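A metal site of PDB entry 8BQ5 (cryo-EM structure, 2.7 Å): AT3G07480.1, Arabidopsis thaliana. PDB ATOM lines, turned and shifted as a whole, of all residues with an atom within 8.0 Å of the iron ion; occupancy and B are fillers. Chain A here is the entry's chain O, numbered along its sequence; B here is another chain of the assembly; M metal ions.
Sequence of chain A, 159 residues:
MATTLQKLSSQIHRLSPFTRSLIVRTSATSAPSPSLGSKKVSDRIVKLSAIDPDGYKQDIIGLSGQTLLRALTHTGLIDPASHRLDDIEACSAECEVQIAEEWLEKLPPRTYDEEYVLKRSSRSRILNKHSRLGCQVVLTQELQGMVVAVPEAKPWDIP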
ATOM      1  N   LEU A  69      -9.104 -22.476 -30.292  1.00  0.00           N
ATOM      2  CA  LEU A  69      -9.717 -22.728 -28.994  1.00  0.00           C
ATOM      3  C   LEU A  69     -10.936 -21.849 -28.780  1.00  0.00           C
ATOM      4  O   LEU A  69     -11.955 -22.313 -28.244  1.00  0.00           O
ATOM      5  CB  LEU A  69      -8.695 -22.497 -27.875  1.00  0.00           C
ATOM      6  CG  LEU A  69      -9.258 -22.392 -26.464  1.00  0.00           C
ATOM      7  CD1 LEU A  69      -9.892 -23.707 -26.023  1.00  0.00           C
ATOM      8  CD2 LEU A  69      -8.195 -21.947 -25.478  1.00  0.00           C
ATOM      9  N   SER A  82     -12.183 -24.208 -18.616  1.00  0.00           N
ATOM     10  CA  SER A  82     -11.008 -25.067 -18.538  1.00  0.00           C
ATOM     11  C   SER A  82      -9.771 -24.436 -19.179  1.00  0.00           C
ATOM     12  O   SER A  82      -8.655 -24.904 -18.936  1.00  0.00           O
ATOM     13  CB  SER A  82     -11.291 -26.409 -19.205  1.00  0.00           C
ATOM     14  OG  SER A  82     -11.128 -26.307 -20.606  1.00  0.00           O
ATOM     15  N   HIS A  83      -9.952 -23.406 -20.006  1.00  0.00           N
ATOM     16  CA  HIS A  83      -8.845 -22.766 -20.714  1.00  0.00           C
ATOM     17  C   HIS A  83      -9.243 -21.303 -20.943  1.00  0.00           C
ATOM     18  O   HIS A  83      -9.886 -20.985 -21.941  1.00  0.00           O
ATOM     19  CB  HIS A  83      -8.559 -23.488 -22.020  1.00  0.00           C
ATOM     20  CG  HIS A  83      -7.150 -23.380 -22.498  1.00  0.00           C
ATOM     21  ND1 HIS A  83      -6.422 -22.209 -22.433  1.00  0.00           N
ATOM     22  CD2 HIS A  83      -6.320 -24.300 -23.046  1.00  0.00           C
ATOM     23  CE1 HIS A  83      -5.215 -22.412 -22.923  1.00  0.00           C
ATOM     24  NE2 HIS A  83      -5.126 -23.670 -23.314  1.00  0.00           N
ATOM     25  N   LEU A  85      -7.120 -18.451 -20.866  1.00  0.00           N
ATOM     26  CA  LEU A  85      -6.151 -17.631 -21.580  1.00  0.00           C
ATOM     27  C   LEU A  85      -5.658 -18.370 -22.809  1.00  0.00           C
ATOM     28  O   LEU A  85      -5.673 -19.604 -22.866  1.00  0.00           O
ATOM     29  CB  LEU A  85      -4.960 -17.274 -20.675  1.00  0.00           C
ATOM     30  CG  LEU A  85      -5.259 -16.727 -19.272  1.00  0.00           C
ATOM     31  CD1 LEU A  85      -3.973 -16.284 -18.607  1.00  0.00           C
ATOM     32  CD2 LEU A  85      -6.262 -15.587 -19.321  1.00  0.00           C
ATOM     33  N   ASP A  86      -5.209 -17.611 -23.808  1.00  0.00           N
ATOM     34  CA  ASP A  86      -4.623 -18.178 -25.029  1.00  0.00           C
ATOM     35  C   ASP A  86      -3.106 -18.244 -24.947  1.00  0.00           C
ATOM     36  O   ASP A  86      -2.417 -18.020 -25.941  1.00  0.00           O
ATOM     37  CB  ASP A  86      -5.049 -17.377 -26.259  1.00  0.00           C
ATOM     38  CG  ASP A  86      -6.471 -17.668 -26.682  1.00  0.00           C
ATOM     39  OD1 ASP A  86      -6.804 -18.847 -26.921  1.00  0.00           O
ATOM     40  OD2 ASP A  86      -7.262 -16.707 -26.799  1.00  0.00           O
ATOM     41  N   ASP A  87      -2.571 -18.537 -23.772  1.00  0.00           N
ATOM     42  CA  ASP A  87      -1.143 -18.510 -23.513  1.00  0.00           C
ATOM     43  C   ASP A  87      -0.619 -19.930 -23.356  1.00  0.00           C
ATOM     44  O   ASP A  87      -1.305 -20.795 -22.801  1.00  0.00           O
ATOM     45  CB  ASP A  87      -0.853 -17.663 -22.267  1.00  0.00           C
ATOM     46  CG  ASP A  87       0.617 -17.653 -21.873  1.00  0.00           C
ATOM     47  OD1 ASP A  87       1.463 -18.318 -22.501  1.00  0.00           O
ATOM     48  OD2 ASP A  87       0.921 -16.938 -20.895  1.00  0.00           O
ATOM     49  N   ILE A  88       0.591 -20.164 -23.852  1.00  0.00           N
ATOM     50  CA  ILE A  88       1.212 -21.481 -23.729  1.00  0.00           C
ATOM     51  C   ILE A  88       1.589 -21.761 -22.282  1.00  0.00           C
ATOM     52  O   ILE A  88       1.704 -22.921 -21.868  1.00  0.00           O
ATOM     53  CB  ILE A  88       2.430 -21.582 -24.673  1.00  0.00           C
ATOM     54  CG1 ILE A  88       2.971 -23.008 -24.702  1.00  0.00           C
ATOM     55  CG2 ILE A  88       3.533 -20.616 -24.256  1.00  0.00           C
ATOM     56  CD1 ILE A  88       1.949 -24.015 -25.115  1.00  0.00           C
ATOM     57  N   GLU A  89       1.763 -20.715 -21.470  1.00  0.00           N
ATOM     58  CA  GLU A  89       2.115 -20.890 -20.068  1.00  0.00           C
ATOM     59  C   GLU A  89       0.901 -21.153 -19.184  1.00  0.00           C
ATOM     60  O   GLU A  89       1.065 -21.402 -17.990  1.00  0.00           O
ATOM     61  CB  GLU A  89       2.874 -19.662 -19.555  1.00  0.00           C
ATOM     62  CG  GLU A  89       3.932 -19.158 -20.518  1.00  0.00           C
ATOM     63  CD  GLU A  89       5.295 -19.722 -20.202  1.00  0.00           C
ATOM     64  OE1 GLU A  89       5.668 -19.777 -19.011  1.00  0.00           O
ATOM     65  OE2 GLU A  89       6.001 -20.142 -21.156  1.00  0.00           O
ATOM     66  N   ALA A  90      -0.303 -21.083 -19.737  1.00  0.00           N
ATOM     67  CA  ALA A  90      -1.526 -21.449 -19.023  1.00  0.00           C
ATOM     68  C   ALA A  90      -2.238 -22.578 -19.751  1.00  0.00           C
ATOM     69  O   ALA A  90      -3.459 -22.558 -19.948  1.00  0.00           O
ATOM     70  CB  ALA A  90      -2.436 -20.230 -18.864  1.00  0.00           C
ATOM     71  N   CYS A  91      -1.471 -23.585 -20.172  1.00  0.00           N
ATOM     72  CA  CYS A  91      -1.994 -24.679 -20.965  1.00  0.00           C
ATOM     73  C   CYS A  91      -1.509 -26.011 -20.389  1.00  0.00           C
ATOM     74  O   CYS A  91      -0.313 -26.185 -20.154  1.00  0.00           O
ATOM     75  CB  CYS A  91      -1.535 -24.548 -22.427  1.00  0.00           C
ATOM     76  SG  CYS A  91      -1.992 -25.938 -23.482  1.00  0.00           S
ATOM     77  N   SER A  92      -2.446 -26.923 -20.171  1.00  0.00           N
ATOM     78  CA  SER A  92      -2.151 -28.317 -19.847  1.00  0.00           C
ATOM     79  C   SER A  92      -2.767 -29.231 -20.888  1.00  0.00           C
ATOM     80  O   SER A  92      -3.260 -30.314 -20.583  1.00  0.00           O
ATOM     81  CB  SER A  92      -2.636 -28.676 -18.442  1.00  0.00           C
ATOM     82  OG  SER A  92      -1.870 -28.026 -17.450  1.00  0.00           O
ATOM     83  N   ALA A  93      -2.768 -28.778 -22.143  1.00  0.00           N
ATOM     84  CA  ALA A  93      -3.379 -29.474 -23.278  1.00  0.00           C
ATOM     85  C   ALA A  93      -4.880 -29.672 -23.095  1.00  0.00           C
ATOM     86  O   ALA A  93      -5.446 -30.609 -23.665  1.00  0.00           O
ATOM     87  CB  ALA A  93      -2.694 -30.818 -23.542  1.00  0.00           C
ATOM     88  N   GLU A  94      -5.537 -28.795 -22.328  1.00  0.00           N
ATOM     89  CA  GLU A  94      -6.994 -28.789 -22.324  1.00  0.00           C
ATOM     90  C   GLU A  94      -7.547 -28.416 -23.694  1.00  0.00           C
ATOM     91  O   GLU A  94      -8.664 -28.826 -24.030  1.00  0.00           O
ATOM     92  CB  GLU A  94      -7.516 -27.795 -21.278  1.00  0.00           C
ATOM     93  CG  GLU A  94      -7.083 -28.075 -19.856  1.00  0.00           C
ATOM     94  CD  GLU A  94      -5.811 -27.334 -19.478  1.00  0.00           C
ATOM     95  OE1 GLU A  94      -5.142 -26.789 -20.372  1.00  0.00           O
ATOM     96  OE2 GLU A  94      -5.499 -27.292 -18.273  1.00  0.00           O
ATOM     97  N   CYS A  95      -6.782 -27.674 -24.477  1.00  0.00           N
ATOM     98  CA  CYS A  95      -7.170 -27.228 -25.809  1.00  0.00           C
ATOM     99  C   CYS A  95      -6.759 -28.202 -26.904  1.00  0.00           C
ATOM    100  O   CYS A  95      -6.922 -27.880 -28.085  1.00  0.00           O
ATOM    101  CB  CYS A  95      -6.555 -25.868 -26.094  1.00  0.00           C
ATOM    102  SG  CYS A  95      -4.761 -25.863 -25.918  1.00  0.00           S
ATOM    103  N   GLU A  96      -6.221 -29.366 -26.547  1.00  0.00           N
ATOM    104  CA  GLU A  96      -5.694 -30.300 -27.536  1.00  0.00           C
ATOM    105  C   GLU A  96      -6.759 -30.698 -28.547  1.00  0.00           C
ATOM    106  O   GLU A  96      -7.897 -30.997 -28.185  1.00  0.00           O
ATOM    107  CB  GLU A  96      -5.146 -31.547 -26.849  1.00  0.00           C
ATOM    108  CG  GLU A  96      -4.014 -32.194 -27.603  1.00  0.00           C
ATOM    109  CD  GLU A  96      -3.929 -33.680 -27.364  1.00  0.00           C
ATOM    110  OE1 GLU A  96      -3.418 -34.091 -26.305  1.00  0.00           O
ATOM    111  OE2 GLU A  96      -4.379 -34.448 -28.248  1.00  0.00           O
ATOM    112  N   VAL A 117       4.418 -29.928 -24.058  1.00  0.00           N
ATOM    113  CA  VAL A 117       3.149 -29.951 -23.348  1.00  0.00           C
ATOM    114  C   VAL A 117       2.311 -31.159 -23.783  1.00  0.00           C
ATOM    115  O   VAL A 117       1.738 -31.868 -22.952  1.00  0.00           O
ATOM    116  CB  VAL A 117       2.382 -28.630 -23.571  1.00  0.00           C
ATOM    117  CG1 VAL A 117       0.909 -28.805 -23.261  1.00  0.00           C
ATOM    118  CG2 VAL A 117       2.986 -27.530 -22.710  1.00  0.00           C
ATOM    119  N   LEU A 118       2.230 -31.396 -25.093  1.00  0.00           N
ATOM    120  CA  LEU A 118       1.424 -32.501 -25.598  1.00  0.00           C
ATOM    121  C   LEU A 118       1.946 -33.837 -25.062  1.00  0.00           C
ATOM    122  O   LEU A 118       1.173 -34.683 -24.598  1.00  0.00           O
ATOM    123  CB  LEU A 118       1.428 -32.505 -27.125  1.00  0.00           C
ATOM    124  CG  LEU A 118       0.800 -31.311 -27.855  1.00  0.00           C
ATOM    125  CD1 LEU A 118       1.149 -31.328 -29.326  1.00  0.00           C
ATOM    126  CD2 LEU A 118      -0.694 -31.338 -27.674  1.00  0.00           C
ATOM    127  N   ARG A 132      -2.499 -31.095 -31.952  1.00  0.00           N
ATOM    128  CA  ARG A 132      -2.137 -29.690 -31.910  1.00  0.00           C
ATOM    129  C   ARG A 132      -2.725 -29.057 -30.665  1.00  0.00           C
ATOM    130  O   ARG A 132      -3.758 -29.499 -30.147  1.00  0.00           O
ATOM    131  CB  ARG A 132      -2.649 -28.936 -33.149  1.00  0.00           C
ATOM    132  CG  ARG A 132      -2.178 -29.518 -34.460  1.00  0.00           C
ATOM    133  CD  ARG A 132      -0.686 -29.313 -34.634  1.00  0.00           C
ATOM    134  NE  ARG A 132      -0.289 -27.946 -34.307  1.00  0.00           N
ATOM    135  CZ  ARG A 132       0.274 -27.109 -35.166  1.00  0.00           C
ATOM    136  NH1 ARG A 132       0.547 -27.468 -36.407  1.00  0.00           N
ATOM    137  NH2 ARG A 132       0.581 -25.878 -34.762  1.00  0.00           N
ATOM    138  N   LEU A 133      -2.054 -28.022 -30.162  1.00  0.00           N
ATOM    139  CA  LEU A 133      -2.589 -27.230 -29.074  1.00  0.00           C
ATOM    140  C   LEU A 133      -3.509 -26.160 -29.666  1.00  0.00           C
ATOM    141  O   LEU A 133      -3.041 -25.269 -30.379  1.00  0.00           O
ATOM    142  CB  LEU A 133      -1.464 -26.587 -28.257  1.00  0.00           C
ATOM    143  CG  LEU A 133      -0.704 -27.513 -27.319  1.00  0.00           C
ATOM    144  CD1 LEU A 133       0.408 -26.766 -26.634  1.00  0.00           C
ATOM    145  CD2 LEU A 133      -1.641 -28.119 -26.281  1.00  0.00           C
ATOM    146  N   GLY A 134      -4.805 -26.251 -29.360  1.00  0.00           N
ATOM    147  CA  GLY A 134      -5.764 -25.343 -29.964  1.00  0.00           C
ATOM    148  C   GLY A 134      -5.506 -23.887 -29.641  1.00  0.00           C
ATOM    149  O   GLY A 134      -5.874 -23.005 -30.427  1.00  0.00           O
ATOM    150  N   CYS A 135      -4.877 -23.612 -28.502  1.00  0.00           N
ATOM    151  CA  CYS A 135      -4.584 -22.232 -28.125  1.00  0.00           C
ATOM    152  C   CYS A 135      -3.459 -21.626 -28.943  1.00  0.00           C
ATOM    153  O   CYS A 135      -3.272 -20.407 -28.916  1.00  0.00           O
ATOM    154  CB  CYS A 135      -4.240 -22.161 -26.632  1.00  0.00           C
ATOM    155  SG  CYS A 135      -2.641 -22.878 -26.200  1.00  0.00           S
ATOM    156  N   GLN A 136      -2.705 -22.446 -29.676  1.00  0.00           N
ATOM    157  CA  GLN A 136      -1.605 -21.967 -30.508  1.00  0.00           C
ATOM    158  C   GLN A 136      -1.947 -21.911 -31.984  1.00  0.00           C
ATOM    159  O   GLN A 136      -1.170 -21.373 -32.768  1.00  0.00           O
ATOM    160  CB  GLN A 136      -0.367 -22.843 -30.297  1.00  0.00           C
ATOM    161  CG  GLN A 136       0.093 -22.934 -28.852  1.00  0.00           C
ATOM    162  CD  GLN A 136       0.511 -21.585 -28.298  1.00  0.00           C
ATOM    163  OE1 GLN A 136       1.514 -21.015 -28.711  1.00  0.00           O
ATOM    164  NE2 GLN A 136      -0.262 -21.082 -27.345  1.00  0.00           N
ATOM    165  N   TYR B 373      -2.674 -21.174 -12.736  1.00  0.00           N
ATOM    166  CA  TYR B 373      -1.366 -20.935 -13.325  1.00  0.00           C
ATOM    167  C   TYR B 373      -0.782 -19.625 -12.822  1.00  0.00           C
ATOM    168  O   TYR B 373      -1.508 -18.736 -12.374  1.00  0.00           O
ATOM    169  CB  TYR B 373      -1.442 -20.899 -14.855  1.00  0.00           C
ATOM    170  CG  TYR B 373      -1.969 -22.166 -15.490  1.00  0.00           C
ATOM    171  CD1 TYR B 373      -1.132 -23.250 -15.684  1.00  0.00           C
ATOM    172  CD2 TYR B 373      -3.291 -22.255 -15.921  1.00  0.00           C
ATOM    173  CE1 TYR B 373      -1.600 -24.409 -16.272  1.00  0.00           C
ATOM    174  CE2 TYR B 373      -3.758 -23.406 -16.504  1.00  0.00           C
ATOM    175  CZ  TYR B 373      -2.915 -24.485 -16.686  1.00  0.00           C
ATOM    176  OH  TYR B 373      -3.382 -25.635 -17.269  1.00  0.00           O
HETATM  177 FE    FE M   1      -3.469 -24.538 -24.606  1.00  0.00          FE
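The backbone carbonyl oxygen (O) of Cys 95 sits at hydrogen-bond distance from the backbone NH (N) of Gly 134 (3.0 Å).
A ring nitrogen (ND1) of His 83 lies within hydrogen-bond range of the backbone carbonyl oxygen of Leu 85 (2.7 Å).
The side-chain sulfur (SG) of Cys 91 sits close to the backbone NH (N) of Ala 93.
The side-chain sulfur (SG) of Cys 135 lies close to the side-chain amide nitrogen (NE2) of Gln 136 (3.2 Å).
Four residues have an atom within 4 Å of the iron ion: His 83, Cys 91, Cys 95 and Cys 135.
The iron ion is bound by the side-chain sulfur (SG) of Cys 95, a ring nitrogen (NE2) of His 83, the side-chain sulfur (SG) of Cys 91 and the side-chain sulfur (SG) of Cys 135.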
